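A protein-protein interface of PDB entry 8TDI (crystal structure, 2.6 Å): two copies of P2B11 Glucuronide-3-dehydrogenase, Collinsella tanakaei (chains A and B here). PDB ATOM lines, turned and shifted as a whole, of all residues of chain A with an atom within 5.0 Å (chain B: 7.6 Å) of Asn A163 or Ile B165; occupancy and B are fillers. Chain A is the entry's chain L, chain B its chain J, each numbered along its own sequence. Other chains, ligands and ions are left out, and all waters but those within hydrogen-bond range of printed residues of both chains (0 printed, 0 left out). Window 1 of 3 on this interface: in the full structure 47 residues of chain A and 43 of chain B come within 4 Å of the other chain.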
ATOM      1  N   ARG A 161      -8.814  23.939 -31.958  1.00  0.00           N
ATOM      2  CA  ARG A 161      -7.898  24.948 -31.454  1.00  0.00           C
ATOM      3  C   ARG A 161      -6.953  25.386 -32.563  1.00  0.00           C
ATOM      4  O   ARG A 161      -6.585  24.578 -33.414  1.00  0.00           O
ATOM      5  CB  ARG A 161      -7.058  24.395 -30.295  1.00  0.00           C
ATOM      6  CG  ARG A 161      -6.315  25.468 -29.512  1.00  0.00           C
ATOM      7  CD  ARG A 161      -5.257  24.942 -28.571  1.00  0.00           C
ATOM      8  NE  ARG A 161      -5.765  23.766 -27.870  1.00  0.00           N
ATOM      9  CZ  ARG A 161      -6.698  23.772 -26.941  1.00  0.00           C
ATOM     10  NH1 ARG A 161      -7.250  22.629 -26.593  1.00  0.00           N
ATOM     11  NH2 ARG A 161      -7.106  24.914 -26.423  1.00  0.00           N
ATOM     12  N   SER A 162      -6.560  26.663 -32.535  1.00  0.00           N
ATOM     13  CA  SER A 162      -5.450  27.125 -33.353  1.00  0.00           C
ATOM     14  C   SER A 162      -4.539  27.965 -32.472  1.00  0.00           C
ATOM     15  O   SER A 162      -4.998  28.586 -31.505  1.00  0.00           O
ATOM     16  CB  SER A 162      -5.903  27.892 -34.565  1.00  0.00           C
ATOM     17  OG  SER A 162      -6.964  28.818 -34.274  1.00  0.00           O
ATOM     18  N   ASN A 163      -3.241  27.909 -32.777  1.00  0.00           N
ATOM     19  CA  ASN A 163      -2.279  28.704 -32.057  1.00  0.00           C
ATOM     20  C   ASN A 163      -1.197  29.079 -33.050  1.00  0.00           C
ATOM     21  O   ASN A 163      -0.613  28.200 -33.678  1.00  0.00           O
ATOM     22  CB  ASN A 163      -1.727  27.976 -30.828  1.00  0.00           C
ATOM     23  CG  ASN A 163      -0.592  28.743 -30.155  1.00  0.00           C
ATOM     24  OD1 ASN A 163      -0.729  29.864 -29.624  1.00  0.00           O
ATOM     25  ND2 ASN A 163       0.619  28.273 -30.400  1.00  0.00           N
ATOM     26  N   TRP A 164      -0.933  30.380 -33.191  1.00  0.00           N
ATOM     27  CA  TRP A 164       0.153  30.798 -34.049  1.00  0.00           C
ATOM     28  C   TRP A 164       1.042  31.768 -33.283  1.00  0.00           C
ATOM     29  O   TRP A 164       0.570  32.833 -32.891  1.00  0.00           O
ATOM     30  CB  TRP A 164      -0.406  31.453 -35.310  1.00  0.00           C
ATOM     31  CG  TRP A 164       0.579  31.549 -36.437  1.00  0.00           C
ATOM     32  CD1 TRP A 164       1.933  31.459 -36.381  1.00  0.00           C
ATOM     33  CD2 TRP A 164       0.242  31.749 -37.823  1.00  0.00           C
ATOM     34  NE1 TRP A 164       2.466  31.598 -37.637  1.00  0.00           N
ATOM     35  CE2 TRP A 164       1.454  31.778 -38.542  1.00  0.00           C
ATOM     36  CE3 TRP A 164      -0.961  31.913 -38.514  1.00  0.00           C
ATOM     37  CZ2 TRP A 164       1.495  31.954 -39.916  1.00  0.00           C
ATOM     38  CZ3 TRP A 164      -0.924  32.088 -39.874  1.00  0.00           C
ATOM     39  CH2 TRP A 164       0.287  32.097 -40.562  1.00  0.00           C
ATOM     40  N   ILE A 165       2.293  31.349 -33.039  1.00  0.00           N
ATOM     41  CA  ILE A 165       3.332  32.206 -32.503  1.00  0.00           C
ATOM     42  C   ILE A 165       4.205  32.614 -33.681  1.00  0.00           C
ATOM     43  O   ILE A 165       4.772  31.755 -34.340  1.00  0.00           O
ATOM     44  CB  ILE A 165       4.157  31.457 -31.445  1.00  0.00           C
ATOM     45  CG1 ILE A 165       3.267  30.841 -30.371  1.00  0.00           C
ATOM     46  CG2 ILE A 165       5.239  32.362 -30.842  1.00  0.00           C
ATOM     47  CD1 ILE A 165       4.004  29.923 -29.417  1.00  0.00           C
ATOM     48  N   SER A 245      -5.272  31.376 -30.523  1.00  0.00           N
ATOM     49  CA  SER A 245      -4.340  32.341 -29.973  1.00  0.00           C
ATOM     50  C   SER A 245      -3.390  32.760 -31.083  1.00  0.00           C
ATOM     51  O   SER A 245      -3.142  31.983 -32.009  1.00  0.00           O
ATOM     52  CB  SER A 245      -3.606  31.820 -28.751  1.00  0.00           C
ATOM     53  OG  SER A 245      -3.673  30.409 -28.662  1.00  0.00           O
ATOM     54  N   PHE A 246      -2.921  34.006 -30.977  1.00  0.00           N
ATOM     55  CA  PHE A 246      -1.997  34.580 -31.932  1.00  0.00           C
ATOM     56  C   PHE A 246      -1.051  35.486 -31.155  1.00  0.00           C
ATOM     57  O   PHE A 246      -1.502  36.340 -30.390  1.00  0.00           O
ATOM     58  CB  PHE A 246      -2.813  35.341 -32.983  1.00  0.00           C
ATOM     59  CG  PHE A 246      -1.986  35.828 -34.160  1.00  0.00           C
ATOM     60  CD1 PHE A 246      -1.236  36.996 -34.068  1.00  0.00           C
ATOM     61  CD2 PHE A 246      -1.992  35.138 -35.368  1.00  0.00           C
ATOM     62  CE1 PHE A 246      -0.487  37.444 -35.141  1.00  0.00           C
ATOM     63  CE2 PHE A 246      -1.241  35.595 -36.435  1.00  0.00           C
ATOM     64  CZ  PHE A 246      -0.494  36.747 -36.317  1.00  0.00           C
ATOM     65  N   ILE A 247       0.250  35.272 -31.337  1.00  0.00           N
ATOM     66  CA  ILE A 247       1.261  36.020 -30.615  1.00  0.00           C
ATOM     67  C   ILE A 247       2.269  36.540 -31.628  1.00  0.00           C
ATOM     68  O   ILE A 247       2.763  35.755 -32.429  1.00  0.00           O
ATOM     69  CB  ILE A 247       1.938  35.109 -29.580  1.00  0.00           C
ATOM     70  CG1 ILE A 247       0.967  34.700 -28.482  1.00  0.00           C
ATOM     71  CG2 ILE A 247       3.179  35.782 -28.997  1.00  0.00           C
ATOM     72  CD1 ILE A 247       1.486  33.579 -27.598  1.00  0.00           C
ATOM     73  N   ARG A 258       5.492  29.169 -35.334  1.00  0.00           N
ATOM     74  CA  ARG A 258       4.905  27.850 -35.230  1.00  0.00           C
ATOM     75  C   ARG A 258       3.391  28.019 -35.217  1.00  0.00           C
ATOM     76  O   ARG A 258       2.864  28.741 -34.373  1.00  0.00           O
ATOM     77  CB  ARG A 258       5.453  27.149 -33.983  1.00  0.00           C
ATOM     78  CG  ARG A 258       4.716  25.881 -33.577  1.00  0.00           C
ATOM     79  CD  ARG A 258       5.592  24.877 -32.814  1.00  0.00           C
ATOM     80  NE  ARG A 258       4.794  24.450 -31.671  1.00  0.00           N
ATOM     81  CZ  ARG A 258       3.708  23.702 -31.702  1.00  0.00           C
ATOM     82  NH1 ARG A 258       3.751  22.382 -31.812  1.00  0.00           N
ATOM     83  NH2 ARG A 258       2.584  24.296 -31.324  1.00  0.00           N
ATOM     84  N   PHE A 259       2.719  27.367 -36.176  1.00  0.00           N
ATOM     85  CA  PHE A 259       1.280  27.459 -36.330  1.00  0.00           C
ATOM     86  C   PHE A 259       0.692  26.063 -36.150  1.00  0.00           C
ATOM     87  O   PHE A 259       1.016  25.151 -36.902  1.00  0.00           O
ATOM     88  CB  PHE A 259       1.008  28.059 -37.711  1.00  0.00           C
ATOM     89  CG  PHE A 259      -0.454  28.227 -38.118  1.00  0.00           C
ATOM     90  CD1 PHE A 259      -0.802  28.229 -39.465  1.00  0.00           C
ATOM     91  CD2 PHE A 259      -1.465  28.398 -37.176  1.00  0.00           C
ATOM     92  CE1 PHE A 259      -2.115  28.387 -39.859  1.00  0.00           C
ATOM     93  CE2 PHE A 259      -2.787  28.581 -37.568  1.00  0.00           C
ATOM     94  CZ  PHE A 259      -3.112  28.571 -38.910  1.00  0.00           C
ATOM     95  N   GLU A 260      -0.144  25.912 -35.126  1.00  0.00           N
ATOM     96  CA  GLU A 260      -0.697  24.622 -34.775  1.00  0.00           C
ATOM     97  C   GLU A 260      -2.209  24.708 -34.960  1.00  0.00           C
ATOM     98  O   GLU A 260      -2.841  25.711 -34.603  1.00  0.00           O
ATOM     99  CB  GLU A 260      -0.301  24.279 -33.338  1.00  0.00           C
ATOM    100  CG  GLU A 260      -1.070  23.097 -32.748  1.00  0.00           C
ATOM    101  CD  GLU A 260      -0.614  22.673 -31.359  1.00  0.00           C
ATOM    102  OE1 GLU A 260       0.608  22.728 -31.080  1.00  0.00           O
ATOM    103  OE2 GLU A 260      -1.458  22.249 -30.558  1.00  0.00           O
ATOM    104  N   ASN B 163       5.276  31.224 -22.629  1.00  0.00           N
ATOM    105  CA  ASN B 163       4.158  30.581 -23.289  1.00  0.00           C
ATOM    106  C   ASN B 163       4.274  29.092 -23.006  1.00  0.00           C
ATOM    107  O   ASN B 163       5.310  28.501 -23.281  1.00  0.00           O
ATOM    108  CB  ASN B 163       4.134  30.904 -24.778  1.00  0.00           C
ATOM    109  CG  ASN B 163       3.053  30.147 -25.516  1.00  0.00           C
ATOM    110  OD1 ASN B 163       3.228  28.980 -25.882  1.00  0.00           O
ATOM    111  ND2 ASN B 163       1.943  30.807 -25.797  1.00  0.00           N
ATOM    112  N   TRP B 164       3.233  28.498 -22.433  1.00  0.00           N
ATOM    113  CA  TRP B 164       3.242  27.069 -22.189  1.00  0.00           C
ATOM    114  C   TRP B 164       1.959  26.460 -22.733  1.00  0.00           C
ATOM    115  O   TRP B 164       0.884  26.800 -22.254  1.00  0.00           O
ATOM    116  CB  TRP B 164       3.384  26.802 -20.689  1.00  0.00           C
ATOM    117  CG  TRP B 164       3.811  25.401 -20.357  1.00  0.00           C
ATOM    118  CD1 TRP B 164       3.768  24.294 -21.146  1.00  0.00           C
ATOM    119  CD2 TRP B 164       4.372  24.979 -19.101  1.00  0.00           C
ATOM    120  NE1 TRP B 164       4.261  23.209 -20.466  1.00  0.00           N
ATOM    121  CE2 TRP B 164       4.641  23.599 -19.213  1.00  0.00           C
ATOM    122  CE3 TRP B 164       4.666  25.637 -17.906  1.00  0.00           C
ATOM    123  CZ2 TRP B 164       5.185  22.866 -18.168  1.00  0.00           C
ATOM    124  CZ3 TRP B 164       5.208  24.913 -16.869  1.00  0.00           C
ATOM    125  CH2 TRP B 164       5.477  23.544 -17.008  1.00  0.00           C
ATOM    126  N   ILE B 165       2.093  25.610 -23.753  1.00  0.00           N
ATOM    127  CA  ILE B 165       1.013  24.783 -24.263  1.00  0.00           C
ATOM    128  C   ILE B 165       1.223  23.388 -23.696  1.00  0.00           C
ATOM    129  O   ILE B 165       2.263  22.787 -23.943  1.00  0.00           O
ATOM    130  CB  ILE B 165       1.033  24.757 -25.806  1.00  0.00           C
ATOM    131  CG1 ILE B 165       1.034  26.170 -26.384  1.00  0.00           C
ATOM    132  CG2 ILE B 165      -0.104  23.911 -26.373  1.00  0.00           C
ATOM    133  CD1 ILE B 165       1.263  26.216 -27.883  1.00  0.00           C
ATOM    134  N   ILE B 166       0.252  22.874 -22.942  1.00  0.00           N
ATOM    135  CA  ILE B 166       0.413  21.554 -22.358  1.00  0.00           C
ATOM    136  C   ILE B 166      -0.924  20.827 -22.427  1.00  0.00           C
ATOM    137  O   ILE B 166      -1.765  20.939 -21.536  1.00  0.00           O
ATOM    138  CB  ILE B 166       1.036  21.644 -20.954  1.00  0.00           C
ATOM    139  CG1 ILE B 166       1.179  20.271 -20.323  1.00  0.00           C
ATOM    140  CG2 ILE B 166       0.283  22.608 -20.037  1.00  0.00           C
ATOM    141  CD1 ILE B 166       2.177  20.233 -19.172  1.00  0.00           C
ATOM    142  N   ASN B 167      -1.065  20.060 -23.515  1.00  0.00           N
ATOM    143  CA  ASN B 167      -2.313  19.444 -23.924  1.00  0.00           C
ATOM    144  C   ASN B 167      -2.218  17.922 -23.917  1.00  0.00           C
ATOM    145  O   ASN B 167      -3.154  17.249 -24.350  1.00  0.00           O
ATOM    146  CB  ASN B 167      -2.690  19.867 -25.347  1.00  0.00           C
ATOM    147  CG  ASN B 167      -3.331  21.232 -25.419  1.00  0.00           C
ATOM    148  OD1 ASN B 167      -3.295  21.862 -26.477  1.00  0.00           O
ATOM    149  ND2 ASN B 167      -3.929  21.696 -24.327  1.00  0.00           N
ATOM    150  N   ASN B 168      -1.111  17.372 -23.420  1.00  0.00           N
ATOM    151  CA  ASN B 168      -0.815  15.961 -23.635  1.00  0.00           C
ATOM    152  C   ASN B 168      -1.421  15.050 -22.570  1.00  0.00           C
ATOM    153  O   ASN B 168      -1.145  13.869 -22.583  1.00  0.00           O
ATOM    154  CB  ASN B 168       0.686  15.705 -23.706  1.00  0.00           C
ATOM    155  CG  ASN B 168       1.402  16.072 -22.433  1.00  0.00           C
ATOM    156  OD1 ASN B 168       0.856  16.756 -21.561  1.00  0.00           O
ATOM    157  ND2 ASN B 168       2.641  15.639 -22.310  1.00  0.00           N
ATOM    158  N   TRP B 169      -2.238  15.557 -21.662  1.00  0.00           N
ATOM    159  CA  TRP B 169      -2.874  14.651 -20.706  1.00  0.00           C
ATOM    160  C   TRP B 169      -4.327  14.403 -21.108  1.00  0.00           C
ATOM    161  O   TRP B 169      -5.267  14.955 -20.534  1.00  0.00           O
ATOM    162  CB  TRP B 169      -2.726  15.136 -19.255  1.00  0.00           C
ATOM    163  CG  TRP B 169      -2.815  16.629 -19.110  1.00  0.00           C
ATOM    164  CD1 TRP B 169      -3.711  17.477 -19.696  1.00  0.00           C
ATOM    165  CD2 TRP B 169      -1.949  17.446 -18.309  1.00  0.00           C
ATOM    166  NE1 TRP B 169      -3.463  18.766 -19.304  1.00  0.00           N
ATOM    167  CE2 TRP B 169      -2.393  18.779 -18.454  1.00  0.00           C
ATOM    168  CE3 TRP B 169      -0.870  17.180 -17.459  1.00  0.00           C
ATOM    169  CZ2 TRP B 169      -1.786  19.845 -17.791  1.00  0.00           C
ATOM    170  CZ3 TRP B 169      -0.254  18.251 -16.816  1.00  0.00           C
ATOM    171  CH2 TRP B 169      -0.717  19.554 -16.978  1.00  0.00           C
ATOM    172  N   THR B 233      -7.411  28.704 -21.702  1.00  0.00           N
ATOM    173  CA  THR B 233      -6.398  29.540 -22.309  1.00  0.00           C
ATOM    174  C   THR B 233      -6.235  30.768 -21.428  1.00  0.00           C
ATOM    175  O   THR B 233      -7.218  31.425 -21.139  1.00  0.00           O
ATOM    176  CB  THR B 233      -6.841  29.926 -23.714  1.00  0.00           C
ATOM    177  OG1 THR B 233      -7.093  28.738 -24.461  1.00  0.00           O
ATOM    178  CG2 THR B 233      -5.794  30.753 -24.430  1.00  0.00           C
ATOM    179  N   SER B 245       1.313  33.225 -21.479  1.00  0.00           N
ATOM    180  CA  SER B 245       0.143  32.483 -21.901  1.00  0.00           C
ATOM    181  C   SER B 245       0.295  31.040 -21.456  1.00  0.00           C
ATOM    182  O   SER B 245       1.409  30.563 -21.318  1.00  0.00           O
ATOM    183  CB  SER B 245      -0.111  32.606 -23.392  1.00  0.00           C
ATOM    184  OG  SER B 245       1.049  33.043 -24.088  1.00  0.00           O
ATOM    185  N   PHE B 246      -0.844  30.403 -21.187  1.00  0.00           N
ATOM    186  CA  PHE B 246      -0.906  29.030 -20.726  1.00  0.00           C
ATOM    187  C   PHE B 246      -2.150  28.400 -21.337  1.00  0.00           C
ATOM    188  O   PHE B 246      -3.227  28.959 -21.223  1.00  0.00           O
ATOM    189  CB  PHE B 246      -0.923  29.025 -19.198  1.00  0.00           C
ATOM    190  CG  PHE B 246      -0.804  27.650 -18.573  1.00  0.00           C
ATOM    191  CD1 PHE B 246      -1.913  26.803 -18.478  1.00  0.00           C
ATOM    192  CD2 PHE B 246       0.397  27.220 -18.042  1.00  0.00           C
ATOM    193  CE1 PHE B 246      -1.806  25.550 -17.918  1.00  0.00           C
ATOM    194  CE2 PHE B 246       0.498  25.960 -17.469  1.00  0.00           C
ATOM    195  CZ  PHE B 246      -0.609  25.134 -17.405  1.00  0.00           C
ATOM    196  N   ILE B 247      -1.981  27.256 -21.994  1.00  0.00           N
ATOM    197  CA  ILE B 247      -3.069  26.576 -22.662  1.00  0.00           C
ATOM    198  C   ILE B 247      -3.046  25.117 -22.224  1.00  0.00           C
ATOM    199  O   ILE B 247      -1.998  24.492 -22.314  1.00  0.00           O
ATOM    200  CB  ILE B 247      -2.899  26.696 -24.182  1.00  0.00           C
ATOM    201  CG1 ILE B 247      -2.986  28.124 -24.658  1.00  0.00           C
ATOM    202  CG2 ILE B 247      -3.891  25.792 -24.904  1.00  0.00           C
ATOM    203  CD1 ILE B 247      -2.540  28.297 -26.109  1.00  0.00           C
ATOM    204  N   THR B 248      -4.187  24.555 -21.811  1.00  0.00           N
ATOM    205  CA  THR B 248      -4.227  23.145 -21.451  1.00  0.00           C
ATOM    206  C   THR B 248      -5.636  22.601 -21.660  1.00  0.00           C
ATOM    207  O   THR B 248      -6.602  23.353 -21.570  1.00  0.00           O
ATOM    208  CB  THR B 248      -3.745  22.960 -20.008  1.00  0.00           C
ATOM    209  OG1 THR B 248      -3.648  21.561 -19.756  1.00  0.00           O
ATOM    210  CG2 THR B 248      -4.669  23.581 -18.984  1.00  0.00           C
ATOM    211  N   CYS B 249      -5.745  21.297 -21.919  1.00  0.00           N
ATOM    212  CA  CYS B 249      -7.044  20.670 -22.081  1.00  0.00           C
ATOM    213  C   CYS B 249      -6.893  19.152 -21.975  1.00  0.00           C
ATOM    214  O   CYS B 249      -5.781  18.635 -22.014  1.00  0.00           O
ATOM    215  CB  CYS B 249      -7.667  21.059 -23.417  1.00  0.00           C
ATOM    216  SG  CYS B 249      -7.158  19.976 -24.785  1.00  0.00           S
ATOM    217  N   ASP B 252      -7.266  16.457 -26.160  1.00  0.00           N
ATOM    218  CA  ASP B 252      -6.315  16.439 -27.263  1.00  0.00           C
ATOM    219  C   ASP B 252      -5.616  15.082 -27.291  1.00  0.00           C
ATOM    220  O   ASP B 252      -4.852  14.760 -26.386  1.00  0.00           O
ATOM    221  CB  ASP B 252      -5.325  17.585 -27.156  1.00  0.00           C
ATOM    222  CG  ASP B 252      -4.499  17.889 -28.391  1.00  0.00           C
ATOM    223  OD1 ASP B 252      -4.316  16.975 -29.212  1.00  0.00           O
ATOM    224  OD2 ASP B 252      -4.068  19.054 -28.536  1.00  0.00           O
ATOM    225  N   GLY B 255      -1.337  15.950 -27.823  1.00  0.00           N
ATOM    226  CA  GLY B 255      -1.231  17.308 -27.338  1.00  0.00           C
ATOM    227  C   GLY B 255       0.219  17.765 -27.307  1.00  0.00           C
ATOM    228  O   GLY B 255       1.096  17.025 -26.893  1.00  0.00           O
ATOM    229  N   THR B 256       0.441  19.001 -27.759  1.00  0.00           N
ATOM    230  CA  THR B 256       1.712  19.661 -27.588  1.00  0.00           C
ATOM    231  C   THR B 256       2.003  19.842 -26.097  1.00  0.00           C
ATOM    232  O   THR B 256       1.084  20.058 -25.309  1.00  0.00           O
ATOM    233  CB  THR B 256       1.621  20.998 -28.309  1.00  0.00           C
ATOM    234  OG1 THR B 256       1.480  20.716 -29.705  1.00  0.00           O
ATOM    235  CG2 THR B 256       2.853  21.850 -28.080  1.00  0.00           C
ATOM    236  N   ASP B 257       3.297  19.741 -25.731  1.00  0.00           N
ATOM    237  CA  ASP B 257       3.813  20.172 -24.440  1.00  0.00           C
ATOM    238  C   ASP B 257       5.071  20.977 -24.718  1.00  0.00           C
ATOM    239  O   ASP B 257       6.143  20.404 -24.837  1.00  0.00           O
ATOM    240  CB  ASP B 257       4.121  18.995 -23.516  1.00  0.00           C
ATOM    241  CG  ASP B 257       4.789  19.320 -22.176  1.00  0.00           C
ATOM    242  OD1 ASP B 257       5.021  20.531 -21.870  1.00  0.00           O
ATOM    243  OD2 ASP B 257       5.107  18.356 -21.437  1.00  0.00           O
ATOM    244  N   ARG B 258       4.933  22.297 -24.855  1.00  0.00           N
ATOM    245  CA  ARG B 258       6.039  23.156 -25.241  1.00  0.00           C
ATOM    246  C   ARG B 258       5.993  24.404 -24.371  1.00  0.00           C
ATOM    247  O   ARG B 258       4.973  25.077 -24.346  1.00  0.00           O
ATOM    248  CB  ARG B 258       5.931  23.451 -26.738  1.00  0.00           C
ATOM    249  CG  ARG B 258       6.862  24.551 -27.239  1.00  0.00           C
ATOM    250  CD  ARG B 258       7.329  24.388 -28.703  1.00  0.00           C
ATOM    251  NE  ARG B 258       7.153  25.718 -29.285  1.00  0.00           N
ATOM    252  CZ  ARG B 258       7.886  26.785 -29.040  1.00  0.00           C
ATOM    253  NH1 ARG B 258       9.058  26.997 -29.603  1.00  0.00           N
ATOM    254  NH2 ARG B 258       7.296  27.784 -28.432  1.00  0.00           N
ATOM    255  N   PHE B 259       7.091  24.668 -23.648  1.00  0.00           N
ATOM    256  CA  PHE B 259       7.191  25.795 -22.737  1.00  0.00           C
ATOM    257  C   PHE B 259       8.319  26.699 -23.210  1.00  0.00           C
ATOM    258  O   PHE B 259       9.460  26.280 -23.277  1.00  0.00           O
ATOM    259  CB  PHE B 259       7.406  25.226 -21.330  1.00  0.00           C
ATOM    260  CG  PHE B 259       7.573  26.226 -20.191  1.00  0.00           C
ATOM    261  CD1 PHE B 259       8.280  25.867 -19.052  1.00  0.00           C
ATOM    262  CD2 PHE B 259       7.011  27.500 -20.242  1.00  0.00           C
ATOM    263  CE1 PHE B 259       8.442  26.761 -18.004  1.00  0.00           C
ATOM    264  CE2 PHE B 259       7.149  28.386 -19.183  1.00  0.00           C
ATOM    265  CZ  PHE B 259       7.874  28.020 -18.073  1.00  0.00           C
ATOM    266  N   GLU B 260       7.980  27.933 -23.561  1.00  0.00           N
ATOM    267  CA  GLU B 260       8.938  28.877 -24.112  1.00  0.00           C
ATOM    268  C   GLU B 260       9.063  30.046 -23.147  1.00  0.00           C
ATOM    269  O   GLU B 260       8.070  30.509 -22.604  1.00  0.00           O
ATOM    270  CB  GLU B 260       8.474  29.315 -25.503  1.00  0.00           C
ATOM    271  CG  GLU B 260       9.254  30.497 -26.075  1.00  0.00           C
ATOM    272  CD  GLU B 260       8.885  30.863 -27.508  1.00  0.00           C
ATOM    273  OE1 GLU B 260       8.642  29.924 -28.302  1.00  0.00           O
ATOM    274  OE2 GLU B 260       8.873  32.070 -27.847  1.00  0.00           O
ATOM    275  N   VAL B 270      11.344  24.304 -23.765  1.00  0.00           N
ATOM    276  CA  VAL B 270      11.319  23.020 -23.107  1.00  0.00           C
ATOM    277  C   VAL B 270      10.286  22.155 -23.791  1.00  0.00           C
ATOM    278  O   VAL B 270       9.118  22.506 -23.785  1.00  0.00           O
ATOM    279  CB  VAL B 270      10.990  23.165 -21.615  1.00  0.00           C
ATOM    280  CG1 VAL B 270      11.068  21.824 -20.903  1.00  0.00           C
ATOM    281  CG2 VAL B 270      11.866  24.214 -20.935  1.00  0.00           C
ATOM    282  N   ASP B 272       8.237  18.551 -24.150  1.00  0.00           N
ATOM    283  CA  ASP B 272       7.745  17.310 -23.579  1.00  0.00           C
ATOM    284  C   ASP B 272       8.150  17.157 -22.118  1.00  0.00           C
ATOM    285  O   ASP B 272       8.077  16.067 -21.569  1.00  0.00           O
ATOM    286  CB  ASP B 272       8.101  16.125 -24.441  1.00  0.00           C
ATOM    287  CG  ASP B 272       7.622  16.245 -25.882  1.00  0.00           C
ATOM    288  OD1 ASP B 272       6.534  16.814 -26.145  1.00  0.00           O
ATOM    289  OD2 ASP B 272       8.439  15.939 -26.743  1.00  0.00           O
ATOM    290  N   SER B 273       8.511  18.273 -21.478  1.00  0.00           N
ATOM    291  CA  SER B 273       8.828  18.284 -20.061  1.00  0.00           C
ATOM    292  C   SER B 273      10.031  17.392 -19.747  1.00  0.00           C
ATOM    293  O   SER B 273      10.207  16.983 -18.600  1.00  0.00           O
ATOM    294  CB  SER B 273       7.624  17.898 -19.231  1.00  0.00           C
ATOM    295  OG  SER B 273       6.656  18.941 -19.236  1.00  0.00           O
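Asn A163 touches Ile B165, and with the chains exchanged Ile A165 touches Asn B163. Ser A245 touches Ile B247, and with the chains exchanged Ile A247 touches Ser B245. Ile A247 touches Asn B163, but with the chains exchanged Asn A163 does not touch Ile B247 (4.3 Å). Arg B258 touches its own counterpart, Arg A258.
The side-chain amide oxygen of Asn B167 lies within hydrogen-bond range of the guanidinium group of Arg A161, at 3.4 Å. NH1 of Arg A161 is in hydrogen-bond range of SG of Cys B249, at 3.2 Å. OE1 of Glu A260 lies within hydrogen-bond range of OG1 of Thr B256, 2.6 Å away.
The backbone carbonyl oxygen (O) of Ser A162 sits at hydrogen-bond distance from the backbone NH (N) of Ser A245. OD1 of Asn A163 sits at hydrogen-bond distance from OG of Ser A245, at 3.1 Å. The backbone NH (N) of Glu A260 sits at hydrogen-bond distance from the backbone carbonyl oxygen (O) of Asn A163 (2.7 Å). The backbone carbonyl oxygen (O) of Ile A165 lies within hydrogen-bond range of the backbone NH (N) of Arg A258 (2.9 Å). The backbone NH of Asn B167 sits at hydrogen-bond distance from the backbone carbonyl oxygen of Thr B256 (2.8 Å). The guanidinium group of Arg B258 is in salt-bridge range of the side-chain carboxylate of Glu B260 (2.5 Å).
Of chain B, only Ile B165 (3.3 Å) comes within 4 Å of Asn A163. Of chain A, only Asn A163 comes within 4 Å of Ile B165. Printed residues of chain A within 4 Å of Thr B256: Arg A258 and Glu A260. Of the printed residues of chain B, Glu A260 touches Thr B256 (2.6 Å). Trp A164 touches none of the printed residues of chain B. The nearest printed residue of chain B that does not touch Arg A258 is Ile B165 (4.2 Å).
Among the printed residues, merely in contact across the chains: Arg A161 with Ile B247 (3.7 Å), Asn A163 with Ile B165 (3.3 Å), Ile A165 with Asn B163 (3.7 Å), Ser A245 with Ile B247 (3.5 Å), Ile A247 with Asn B163 (3.3 Å), Ile A247 with Ser B245 (3.6 Å), Arg A258 with Thr B256 (3.5 Å) and Arg A258 with Arg B258 (3.6 Å).
Printed residues of chain A that touch a printed residue of chain B: Arg A161, Asn A163, Ile A165, Ser A245, Ile A247, Arg A258 and Glu A260. Hydrophobic or aromatic side chains of chain A that line the printed part of chain B: Ile A165 and Ile A247. Among the printed residues, 11 pairs touch across the chains.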
